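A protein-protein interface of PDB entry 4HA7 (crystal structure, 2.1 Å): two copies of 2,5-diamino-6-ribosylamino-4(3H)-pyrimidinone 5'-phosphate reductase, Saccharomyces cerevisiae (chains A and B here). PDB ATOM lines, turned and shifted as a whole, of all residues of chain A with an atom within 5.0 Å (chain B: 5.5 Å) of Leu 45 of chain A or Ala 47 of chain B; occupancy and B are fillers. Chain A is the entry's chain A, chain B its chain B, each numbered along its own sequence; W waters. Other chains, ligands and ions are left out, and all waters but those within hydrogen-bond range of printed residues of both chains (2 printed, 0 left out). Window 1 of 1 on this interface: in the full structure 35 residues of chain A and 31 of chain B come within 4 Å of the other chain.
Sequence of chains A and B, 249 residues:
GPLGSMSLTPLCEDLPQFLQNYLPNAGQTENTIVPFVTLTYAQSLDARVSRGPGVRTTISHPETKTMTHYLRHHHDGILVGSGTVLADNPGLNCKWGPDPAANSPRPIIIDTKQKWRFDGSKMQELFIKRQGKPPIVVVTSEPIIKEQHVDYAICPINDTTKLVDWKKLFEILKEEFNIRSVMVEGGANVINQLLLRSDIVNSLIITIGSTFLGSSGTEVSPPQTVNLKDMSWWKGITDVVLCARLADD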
ATOM      1  N   GLN A  43      -5.349  27.348  11.414  1.00  0.00           N
ATOM      2  CA  GLN A  43      -4.873  26.211  12.195  1.00  0.00           C
ATOM      3  C   GLN A  43      -5.699  24.951  11.962  1.00  0.00           C
ATOM      4  O   GLN A  43      -6.846  24.995  11.504  1.00  0.00           O
ATOM      5  CB  GLN A  43      -4.919  26.546  13.690  1.00  0.00           C
ATOM      6  CG  GLN A  43      -6.350  26.632  14.235  1.00  0.00           C
ATOM      7  CD  GLN A  43      -6.374  26.844  15.754  1.00  0.00           C
ATOM      8  OE1 GLN A  43      -5.486  27.466  16.303  1.00  0.00           O
ATOM      9  NE2 GLN A  43      -7.397  26.326  16.419  1.00  0.00           N
ATOM     10  N   SER A  44      -5.094  23.821  12.300  1.00  0.00           N
ATOM     11  CA  SER A  44      -5.776  22.534  12.331  1.00  0.00           C
ATOM     12  C   SER A  44      -6.655  22.432  13.590  1.00  0.00           C
ATOM     13  O   SER A  44      -6.618  23.308  14.460  1.00  0.00           O
ATOM     14  CB  SER A  44      -4.722  21.422  12.386  1.00  0.00           C
ATOM     15  OG  SER A  44      -3.840  21.683  13.466  1.00  0.00           O
ATOM     16  N   LEU A  45      -7.418  21.346  13.689  1.00  0.00           N
ATOM     17  CA  LEU A  45      -8.220  21.069  14.881  1.00  0.00           C
ATOM     18  C   LEU A  45      -7.342  20.942  16.116  1.00  0.00           C
ATOM     19  O   LEU A  45      -7.764  21.316  17.205  1.00  0.00           O
ATOM     20  CB  LEU A  45      -9.056  19.797  14.713  1.00  0.00           C
ATOM     21  CG  LEU A  45     -10.193  19.911  13.691  1.00  0.00           C
ATOM     22  CD1 LEU A  45     -10.663  18.509  13.289  1.00  0.00           C
ATOM     23  CD2 LEU A  45     -11.331  20.718  14.253  1.00  0.00           C
ATOM     24  N   ASP A  46      -6.120  20.425  15.952  1.00  0.00           N
ATOM     25  CA  ASP A  46      -5.188  20.344  17.089  1.00  0.00           C
ATOM     26  C   ASP A  46      -4.322  21.588  17.265  1.00  0.00           C
ATOM     27  O   ASP A  46      -3.210  21.530  17.807  1.00  0.00           O
ATOM     28  CB  ASP A  46      -4.353  19.046  17.121  1.00  0.00           C
ATOM     29  CG  ASP A  46      -3.789  18.644  15.748  1.00  0.00           C
ATOM     30  OD1 ASP A  46      -4.149  19.273  14.731  1.00  0.00           O
ATOM     31  OD2 ASP A  46      -3.011  17.657  15.692  1.00  0.00           O
ATOM     32  N   ALA A  47      -4.860  22.714  16.804  1.00  0.00           N
ATOM     33  CA  ALA A  47      -4.244  24.019  16.990  1.00  0.00           C
ATOM     34  C   ALA A  47      -2.818  24.069  16.426  1.00  0.00           C
ATOM     35  O   ALA A  47      -1.931  24.701  16.994  1.00  0.00           O
ATOM     36  CB  ALA A  47      -4.261  24.410  18.480  1.00  0.00           C
ATOM     37  N   ILE A 208     -10.130  27.625  11.266  1.00  0.00           N
ATOM     38  CA  ILE A 208      -9.863  26.270  11.761  1.00  0.00           C
ATOM     39  C   ILE A 208     -10.243  25.260  10.692  1.00  0.00           C
ATOM     40  O   ILE A 208     -11.393  25.204  10.277  1.00  0.00           O
ATOM     41  CB  ILE A 208     -10.695  25.962  13.021  1.00  0.00           C
ATOM     42  CG1 ILE A 208     -10.429  27.033  14.073  1.00  0.00           C
ATOM     43  CG2 ILE A 208     -10.390  24.528  13.529  1.00  0.00           C
ATOM     44  CD1 ILE A 208     -11.220  26.860  15.372  1.00  0.00           C
ATOM     45  N   GLY A 209      -9.282  24.470  10.235  1.00  0.00           N
ATOM     46  CA  GLY A 209      -9.562  23.478   9.203  1.00  0.00           C
ATOM     47  C   GLY A 209     -10.015  22.174   9.857  1.00  0.00           C
ATOM     48  O   GLY A 209      -9.657  21.904  10.999  1.00  0.00           O
ATOM     49  N   SER A 210     -10.799  21.372   9.142  1.00  0.00           N
ATOM     50  CA  SER A 210     -11.184  20.052   9.623  1.00  0.00           C
ATOM     51  C   SER A 210     -10.137  18.974   9.317  1.00  0.00           C
ATOM     52  O   SER A 210     -10.339  18.074   8.502  1.00  0.00           O
ATOM     53  CB  SER A 210     -12.587  19.666   9.136  1.00  0.00           C
ATOM     54  OG  SER A 210     -12.746  19.860   7.745  1.00  0.00           O
ATOM     55  N   THR A 211      -9.013  19.064  10.017  1.00  0.00           N
ATOM     56  CA  THR A 211      -7.928  18.128   9.857  1.00  0.00           C
ATOM     57  C   THR A 211      -7.064  18.185  11.109  1.00  0.00           C
ATOM     58  O   THR A 211      -7.063  19.196  11.798  1.00  0.00           O
ATOM     59  CB  THR A 211      -7.055  18.469   8.590  1.00  0.00           C
ATOM     60  OG1 THR A 211      -6.279  17.330   8.206  1.00  0.00           O
ATOM     61  CG2 THR A 211      -6.119  19.639   8.858  1.00  0.00           C
ATOM     62  N   PHE A 212      -6.351  17.093  11.390  1.00  0.00           N
ATOM     63  CA  PHE A 212      -5.314  17.056  12.428  1.00  0.00           C
ATOM     64  C   PHE A 212      -3.939  17.056  11.791  1.00  0.00           C
ATOM     65  O   PHE A 212      -3.662  16.232  10.925  1.00  0.00           O
ATOM     66  CB  PHE A 212      -5.467  15.784  13.282  1.00  0.00           C
ATOM     67  CG  PHE A 212      -6.744  15.744  14.047  1.00  0.00           C
ATOM     68  CD1 PHE A 212      -6.838  16.348  15.300  1.00  0.00           C
ATOM     69  CD2 PHE A 212      -7.869  15.137  13.511  1.00  0.00           C
ATOM     70  CE1 PHE A 212      -8.033  16.331  16.011  1.00  0.00           C
ATOM     71  CE2 PHE A 212      -9.064  15.097  14.224  1.00  0.00           C
ATOM     72  CZ  PHE A 212      -9.149  15.711  15.473  1.00  0.00           C
ATOM     73  N   TYR B  41     -15.590  14.952  22.261  1.00  0.00           N
ATOM     74  CA  TYR B  41     -14.943  15.747  23.289  1.00  0.00           C
ATOM     75  C   TYR B  41     -15.134  17.242  23.058  1.00  0.00           C
ATOM     76  O   TYR B  41     -15.614  17.667  22.004  1.00  0.00           O
ATOM     77  CB  TYR B  41     -13.451  15.408  23.383  1.00  0.00           C
ATOM     78  CG  TYR B  41     -12.603  15.689  22.143  1.00  0.00           C
ATOM     79  CD1 TYR B  41     -11.899  16.888  22.021  1.00  0.00           C
ATOM     80  CD2 TYR B  41     -12.466  14.746  21.130  1.00  0.00           C
ATOM     81  CE1 TYR B  41     -11.096  17.157  20.922  1.00  0.00           C
ATOM     82  CE2 TYR B  41     -11.648  15.002  20.009  1.00  0.00           C
ATOM     83  CZ  TYR B  41     -10.969  16.213  19.922  1.00  0.00           C
ATOM     84  OH  TYR B  41     -10.163  16.497  18.850  1.00  0.00           O
ATOM     85  N   GLN B  43     -13.148  20.948  23.390  1.00  0.00           N
ATOM     86  CA  GLN B  43     -11.824  21.531  23.509  1.00  0.00           C
ATOM     87  C   GLN B  43     -11.880  23.043  23.372  1.00  0.00           C
ATOM     88  O   GLN B  43     -12.896  23.618  22.967  1.00  0.00           O
ATOM     89  CB  GLN B  43     -10.883  20.969  22.448  1.00  0.00           C
ATOM     90  CG  GLN B  43     -11.209  21.467  21.033  1.00  0.00           C
ATOM     91  CD  GLN B  43     -10.233  20.920  20.010  1.00  0.00           C
ATOM     92  OE1 GLN B  43      -9.699  19.825  20.185  1.00  0.00           O
ATOM     93  NE2 GLN B  43      -9.963  21.691  18.958  1.00  0.00           N
ATOM     94  N   SER B  44     -10.772  23.681  23.719  1.00  0.00           N
ATOM     95  CA  SER B  44     -10.646  25.121  23.582  1.00  0.00           C
ATOM     96  C   SER B  44     -10.077  25.378  22.195  1.00  0.00           C
ATOM     97  O   SER B  44      -9.845  24.439  21.433  1.00  0.00           O
ATOM     98  CB  SER B  44      -9.695  25.658  24.643  1.00  0.00           C
ATOM     99  OG  SER B  44      -8.448  24.970  24.585  1.00  0.00           O
ATOM    100  N   LEU B  45      -9.858  26.647  21.862  1.00  0.00           N
ATOM    101  CA  LEU B  45      -9.268  27.000  20.574  1.00  0.00           C
ATOM    102  C   LEU B  45      -7.877  26.390  20.436  1.00  0.00           C
ATOM    103  O   LEU B  45      -7.476  25.973  19.338  1.00  0.00           O
ATOM    104  CB  LEU B  45      -9.190  28.526  20.409  1.00  0.00           C
ATOM    105  CG  LEU B  45     -10.554  29.189  20.166  1.00  0.00           C
ATOM    106  CD1 LEU B  45     -10.490  30.658  20.450  1.00  0.00           C
ATOM    107  CD2 LEU B  45     -10.999  28.954  18.720  1.00  0.00           C
ATOM    108  N   ASP B  46      -7.141  26.343  21.549  1.00  0.00           N
ATOM    109  CA  ASP B  46      -5.833  25.723  21.503  1.00  0.00           C
ATOM    110  C   ASP B  46      -5.837  24.203  21.802  1.00  0.00           C
ATOM    111  O   ASP B  46      -4.853  23.665  22.289  1.00  0.00           O
ATOM    112  CB  ASP B  46      -4.768  26.503  22.288  1.00  0.00           C
ATOM    113  CG  ASP B  46      -5.184  26.837  23.724  1.00  0.00           C
ATOM    114  OD1 ASP B  46      -6.371  26.706  24.100  1.00  0.00           O
ATOM    115  OD2 ASP B  46      -4.294  27.276  24.479  1.00  0.00           O
ATOM    116  N   ALA B  47      -6.935  23.534  21.444  1.00  0.00           N
ATOM    117  CA  ALA B  47      -7.013  22.067  21.438  1.00  0.00           C
ATOM    118  C   ALA B  47      -6.776  21.447  22.804  1.00  0.00           C
ATOM    119  O   ALA B  47      -6.236  20.357  22.913  1.00  0.00           O
ATOM    120  CB  ALA B  47      -6.051  21.465  20.415  1.00  0.00           C
ATOM    121  N   ARG B  48      -7.180  22.154  23.847  1.00  0.00           N
ATOM    122  CA  ARG B  48      -7.024  21.643  25.188  1.00  0.00           C
ATOM    123  C   ARG B  48      -8.344  21.172  25.798  1.00  0.00           C
ATOM    124  O   ARG B  48      -9.392  21.775  25.590  1.00  0.00           O
ATOM    125  CB  ARG B  48      -6.311  22.674  26.065  1.00  0.00           C
ATOM    126  CG  ARG B  48      -4.873  22.258  26.367  1.00  0.00           C
ATOM    127  CD  ARG B  48      -3.827  23.245  25.893  1.00  0.00           C
ATOM    128  NE  ARG B  48      -3.433  23.050  24.503  1.00  0.00           N
ATOM    129  CZ  ARG B  48      -2.177  22.875  24.098  1.00  0.00           C
ATOM    130  NH1 ARG B  48      -1.182  22.860  24.974  1.00  0.00           N
ATOM    131  NH2 ARG B  48      -1.917  22.717  22.809  1.00  0.00           N
ATOM    132  N   VAL B  49      -8.293  20.070  26.540  1.00  0.00           N
ATOM    133  CA  VAL B  49      -9.504  19.537  27.150  1.00  0.00           C
ATOM    134  C   VAL B  49      -9.534  19.769  28.661  1.00  0.00           C
ATOM    135  O   VAL B  49     -10.552  19.548  29.313  1.00  0.00           O
ATOM    136  CB  VAL B  49      -9.685  18.061  26.818  1.00  0.00           C
ATOM    137  CG1 VAL B  49      -9.843  17.904  25.320  1.00  0.00           C
ATOM    138  CG2 VAL B  49      -8.499  17.252  27.329  1.00  0.00           C
ATOM    139  N   LEU B 204     -17.063  11.262  14.661  1.00  0.00           N
ATOM    140  CA  LEU B 204     -16.214  12.117  15.485  1.00  0.00           C
ATOM    141  C   LEU B 204     -16.998  13.393  15.703  1.00  0.00           C
ATOM    142  O   LEU B 204     -17.514  13.958  14.753  1.00  0.00           O
ATOM    143  CB  LEU B 204     -14.874  12.372  14.799  1.00  0.00           C
ATOM    144  CG  LEU B 204     -13.990  13.495  15.358  1.00  0.00           C
ATOM    145  CD1 LEU B 204     -13.423  13.097  16.699  1.00  0.00           C
ATOM    146  CD2 LEU B 204     -12.875  13.844  14.376  1.00  0.00           C
ATOM    147  N   ILE B 206     -16.824  16.974  17.746  1.00  0.00           N
ATOM    148  CA  ILE B 206     -15.941  17.852  18.498  1.00  0.00           C
ATOM    149  C   ILE B 206     -16.582  19.208  18.699  1.00  0.00           C
ATOM    150  O   ILE B 206     -16.998  19.842  17.726  1.00  0.00           O
ATOM    151  CB  ILE B 206     -14.627  18.067  17.742  1.00  0.00           C
ATOM    152  CG1 ILE B 206     -13.982  16.715  17.431  1.00  0.00           C
ATOM    153  CG2 ILE B 206     -13.704  19.019  18.528  1.00  0.00           C
ATOM    154  CD1 ILE B 206     -12.660  16.799  16.704  1.00  0.00           C
ATOM    155  N   ILE B 208     -15.853  23.042  19.851  1.00  0.00           N
ATOM    156  CA  ILE B 208     -14.745  23.956  20.084  1.00  0.00           C
ATOM    157  C   ILE B 208     -15.285  25.238  20.704  1.00  0.00           C
ATOM    158  O   ILE B 208     -16.156  25.895  20.133  1.00  0.00           O
ATOM    159  CB  ILE B 208     -13.997  24.302  18.777  1.00  0.00           C
ATOM    160  CG1 ILE B 208     -13.536  23.032  18.058  1.00  0.00           C
ATOM    161  CG2 ILE B 208     -12.787  25.192  19.070  1.00  0.00           C
ATOM    162  CD1 ILE B 208     -13.027  23.293  16.643  1.00  0.00           C
ATOM    163  N   THR B 218      -3.885  20.015  29.151  1.00  0.00           N
ATOM    164  CA  THR B 218      -3.748  18.735  28.459  1.00  0.00           C
ATOM    165  C   THR B 218      -4.353  18.778  27.055  1.00  0.00           C
ATOM    166  O   THR B 218      -5.548  19.050  26.867  1.00  0.00           O
ATOM    167  CB  THR B 218      -4.335  17.553  29.275  1.00  0.00           C
ATOM    168  OG1 THR B 218      -5.763  17.570  29.197  1.00  0.00           O
ATOM    169  CG2 THR B 218      -3.903  17.645  30.729  1.00  0.00           C
ATOM    170  N   GLU B 219      -3.516  18.505  26.064  1.00  0.00           N
ATOM    171  CA  GLU B 219      -3.930  18.672  24.678  1.00  0.00           C
ATOM    172  C   GLU B 219      -4.516  17.395  24.083  1.00  0.00           C
ATOM    173  O   GLU B 219      -4.238  16.289  24.546  1.00  0.00           O
ATOM    174  CB  GLU B 219      -2.746  19.142  23.821  1.00  0.00           C
ATOM    175  CG  GLU B 219      -1.704  18.055  23.550  1.00  0.00           C
ATOM    176  CD  GLU B 219      -0.757  18.407  22.403  1.00  0.00           C
ATOM    177  OE1 GLU B 219       0.025  17.525  21.973  1.00  0.00           O
ATOM    178  OE2 GLU B 219      -0.790  19.564  21.934  1.00  0.00           O
ATOM    179  N   VAL B 220      -5.338  17.557  23.052  1.00  0.00           N
ATOM    180  CA  VAL B 220      -5.679  16.432  22.210  1.00  0.00           C
ATOM    181  C   VAL B 220      -5.053  16.661  20.841  1.00  0.00           C
ATOM    182  O   VAL B 220      -5.382  17.622  20.139  1.00  0.00           O
ATOM    183  CB  VAL B 220      -7.198  16.209  22.116  1.00  0.00           C
ATOM    184  CG1 VAL B 220      -7.916  17.544  22.103  1.00  0.00           C
ATOM    185  CG2 VAL B 220      -7.551  15.378  20.886  1.00  0.00           C
ATOM    186  N   LEU B 228      -9.883  13.790   7.686  1.00  0.00           N
ATOM    187  CA  LEU B 228     -11.292  13.620   7.981  1.00  0.00           C
ATOM    188  C   LEU B 228     -12.079  13.583   6.690  1.00  0.00           C
ATOM    189  O   LEU B 228     -11.592  13.995   5.640  1.00  0.00           O
ATOM    190  CB  LEU B 228     -11.817  14.766   8.872  1.00  0.00           C
ATOM    191  CG  LEU B 228     -11.302  14.911  10.313  1.00  0.00           C
ATOM    192  CD1 LEU B 228      -9.822  15.208  10.363  1.00  0.00           C
ATOM    193  CD2 LEU B 228     -12.056  16.012  11.036  1.00  0.00           C
ATOM    194  N   TRP B 233     -20.330  21.251   9.926  1.00  0.00           N
ATOM    195  CA  TRP B 233     -20.126  22.182  11.034  1.00  0.00           C
ATOM    196  C   TRP B 233     -21.458  22.748  11.485  1.00  0.00           C
ATOM    197  O   TRP B 233     -22.363  22.952  10.682  1.00  0.00           O
ATOM    198  CB  TRP B 233     -19.211  23.349  10.637  1.00  0.00           C
ATOM    199  CG  TRP B 233     -17.776  23.019  10.451  1.00  0.00           C
ATOM    200  CD1 TRP B 233     -17.149  22.717   9.277  1.00  0.00           C
ATOM    201  CD2 TRP B 233     -16.762  22.997  11.463  1.00  0.00           C
ATOM    202  NE1 TRP B 233     -15.812  22.491   9.503  1.00  0.00           N
ATOM    203  CE2 TRP B 233     -15.546  22.677  10.832  1.00  0.00           C
ATOM    204  CE3 TRP B 233     -16.767  23.208  12.841  1.00  0.00           C
ATOM    205  CZ2 TRP B 233     -14.347  22.564  11.533  1.00  0.00           C
ATOM    206  CZ3 TRP B 233     -15.571  23.100  13.537  1.00  0.00           C
ATOM    207  CH2 TRP B 233     -14.384  22.776  12.886  1.00  0.00           C
ATOM    208  N   LEU B 242     -18.065  20.318  15.286  1.00  0.00           N
ATOM    209  CA  LEU B 242     -17.734  19.583  14.072  1.00  0.00           C
ATOM    210  C   LEU B 242     -18.285  18.164  14.196  1.00  0.00           C
ATOM    211  O   LEU B 242     -18.007  17.484  15.168  1.00  0.00           O
ATOM    212  CB  LEU B 242     -16.212  19.500  13.927  1.00  0.00           C
ATOM    213  CG  LEU B 242     -15.498  19.300  12.585  1.00  0.00           C
ATOM    214  CD1 LEU B 242     -14.352  18.342  12.768  1.00  0.00           C
ATOM    215  CD2 LEU B 242     -16.403  18.870  11.428  1.00  0.00           C
HETATM  216  O   HOH W   1      -9.003  16.283   6.954  1.00  0.00           O
HETATM  217  O   HOH W   2      -9.115  23.976  17.518  1.00  0.00           O
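Of the 10 printed residues of chain A, 8 touch a printed residue of chain B. Hydrophobic or aromatic side chains of chain A within 4 Å of the printed part of chain B: Leu 45, Ala 47, Ile 208 and Phe 212. Along chain A the printed residues that touch a printed residue of chain B span positions 43 to 212. Of the 17 printed residues of chain B, 11 touch a printed residue of chain A. Printed residues of chain B that touch a printed residue of chain A: Tyr 41, Gln 43, Leu 45, Asp 46, Ala 47, Ile 206, Ile 208, Val 220, Leu 228, Trp 233 and Leu 242. Among the printed residues, no Asp or Glu carboxylate lies within 4 Å of a Lys or Arg side-chain nitrogen of the other chain.
Of chain B, only Gln 43 (2.8 Å), Ala 47 (3.6 Å), Ile 208 (3.9 Å), Leu 228 (3.6 Å), Trp 233 (3.9 Å) and Leu 242 (3.7 Å) come within 4 Å of Leu 45 of chain A. Of the printed residues of chain B, Ile 208 of chain A touches Leu 45. Gly 209 of chain A touches none of the printed residues of chain B. Of the printed residues of chain B, Phe 212 of chain A touches Tyr 41 (3.6 Å), Ile 206 (3.9 Å) and Leu 228 (3.7 Å). Ser 44 of chain B touches none of the printed residues of chain A. Ala 47 of chain B touches just these residues of chain A: Leu 45 (3.6 Å), Asp 46 (3.6 Å) and Ala 47 (3.95 Å). Printed residues of chain A within 4 Å of Leu 228 of chain B: Leu 45 (3.6 Å), Ser 210 (3.5 Å), Thr 211 (3.5 Å) and Phe 212 (3.7 Å). Of the printed residues of chain A, Trp 233 of chain B touches Leu 45 (3.9 Å). The nearest residue of chain B that does not touch Leu 45 of chain A is Ile 206 of chain B (4.3 Å). The nearest printed residue of chain B that does not touch Ala 47 of chain A is Arg 48 of chain B (5.2 Å).
The side-chain amide nitrogen of Gln 43 of chain A lies within hydrogen-bond range of the backbone carbonyl oxygen of Leu 45 of chain B (2.9 Å). The side-chain amide nitrogen (NE2) of Gln 43 of chain B lies within hydrogen-bond range of the backbone carbonyl oxygen (O) of Leu 45 of chain A.
The backbone carbonyl oxygen of Gln 43 of chain A lies within hydrogen-bond range of the backbone NH of Gly 209 of chain A (2.8 Å). OD1 of Asp 46 of chain A sits at hydrogen-bond distance from OG of Ser 44 of chain A (2.7 Å). The side-chain hydroxyl of Ser 44 of chain B lies within hydrogen-bond range of the side-chain carboxylate of Asp 46 of chain B (2.8 Å). NE of Arg 48 of chain B is in hydrogen-bond range of O of Asp 46 of chain B (2.7 Å). The backbone carbonyl oxygen (O) of Ala 47 of chain B is in hydrogen-bond range of the backbone NH (N) of Val 220 of chain B (2.9 Å). N of Leu 242 of chain B is in hydrogen-bond range of O of Ile 206 of chain B (2.7 Å).
Water W1 lies within hydrogen-bond range of the backbone carbonyl oxygen of Ser 210 of chain A (2.7 Å), the backbone NH of Leu 228 of chain B (2.7 Å) and the side-chain hydroxyl of Thr 211 of chain A (3.2 Å). Water W2 lies within hydrogen-bond range of the side-chain amide nitrogen of Gln 43 of chain B (2.8 Å), the backbone carbonyl oxygen of Leu 45 of chain A (3.0 Å), the side-chain amide nitrogen of Gln 43 of chain A (3.1 Å) and the backbone carbonyl oxygen of Leu 45 of chain B (3.2 Å).
Ala 47 of chain B touches Leu 45 of chain A (CB to O, 3.6 Å). Leu 228 of chain B touches Leu 45 of chain A. Leu 45 of chain A touches Trp 233 of chain B (CD2 to CH2, 3.9 Å). Leu 45 of chain A touches Leu 242 of chain B. Ala 47 of chain B touches Asp 46 of chain A. CB of Asp 46 of chain A touches O of Val 220 of chain B, at 3.5 Å. Ala 47 of chain A touches Ala 47 of chain B (CB to CB, 3.95 Å). Ile 208 of chain A touches Leu 45 of chain B. CD1 of Ile 206 of chain B touches CZ of Phe 212 of chain A, at 3.9 Å. Phe 212 of chain A touches Leu 228 of chain B (CD2 to CD1, 3.7 Å).
Gln 43 of chain A touches Leu 45 of chain B, and with the chains exchanged Leu 45 of chain A touches Gln 43 of chain B. Leu 45 of chain A touches Ala 47 of chain B, and with the chains exchanged Ala 47 of chain A touches Leu 45 of chain B. Leu 45 of chain A touches Ile 208 of chain B, and with the chains exchanged Ile 208 of chain A touches Leu 45 of chain B. Asp 46 of chain A touches Ala 47 of chain B, and with the chains exchanged Ala 47 of chain A touches Asp 46 of chain B. Of the 18 pairs that touch across the chains among the printed residues, 9 have their exchanged pair printed and touching as well.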
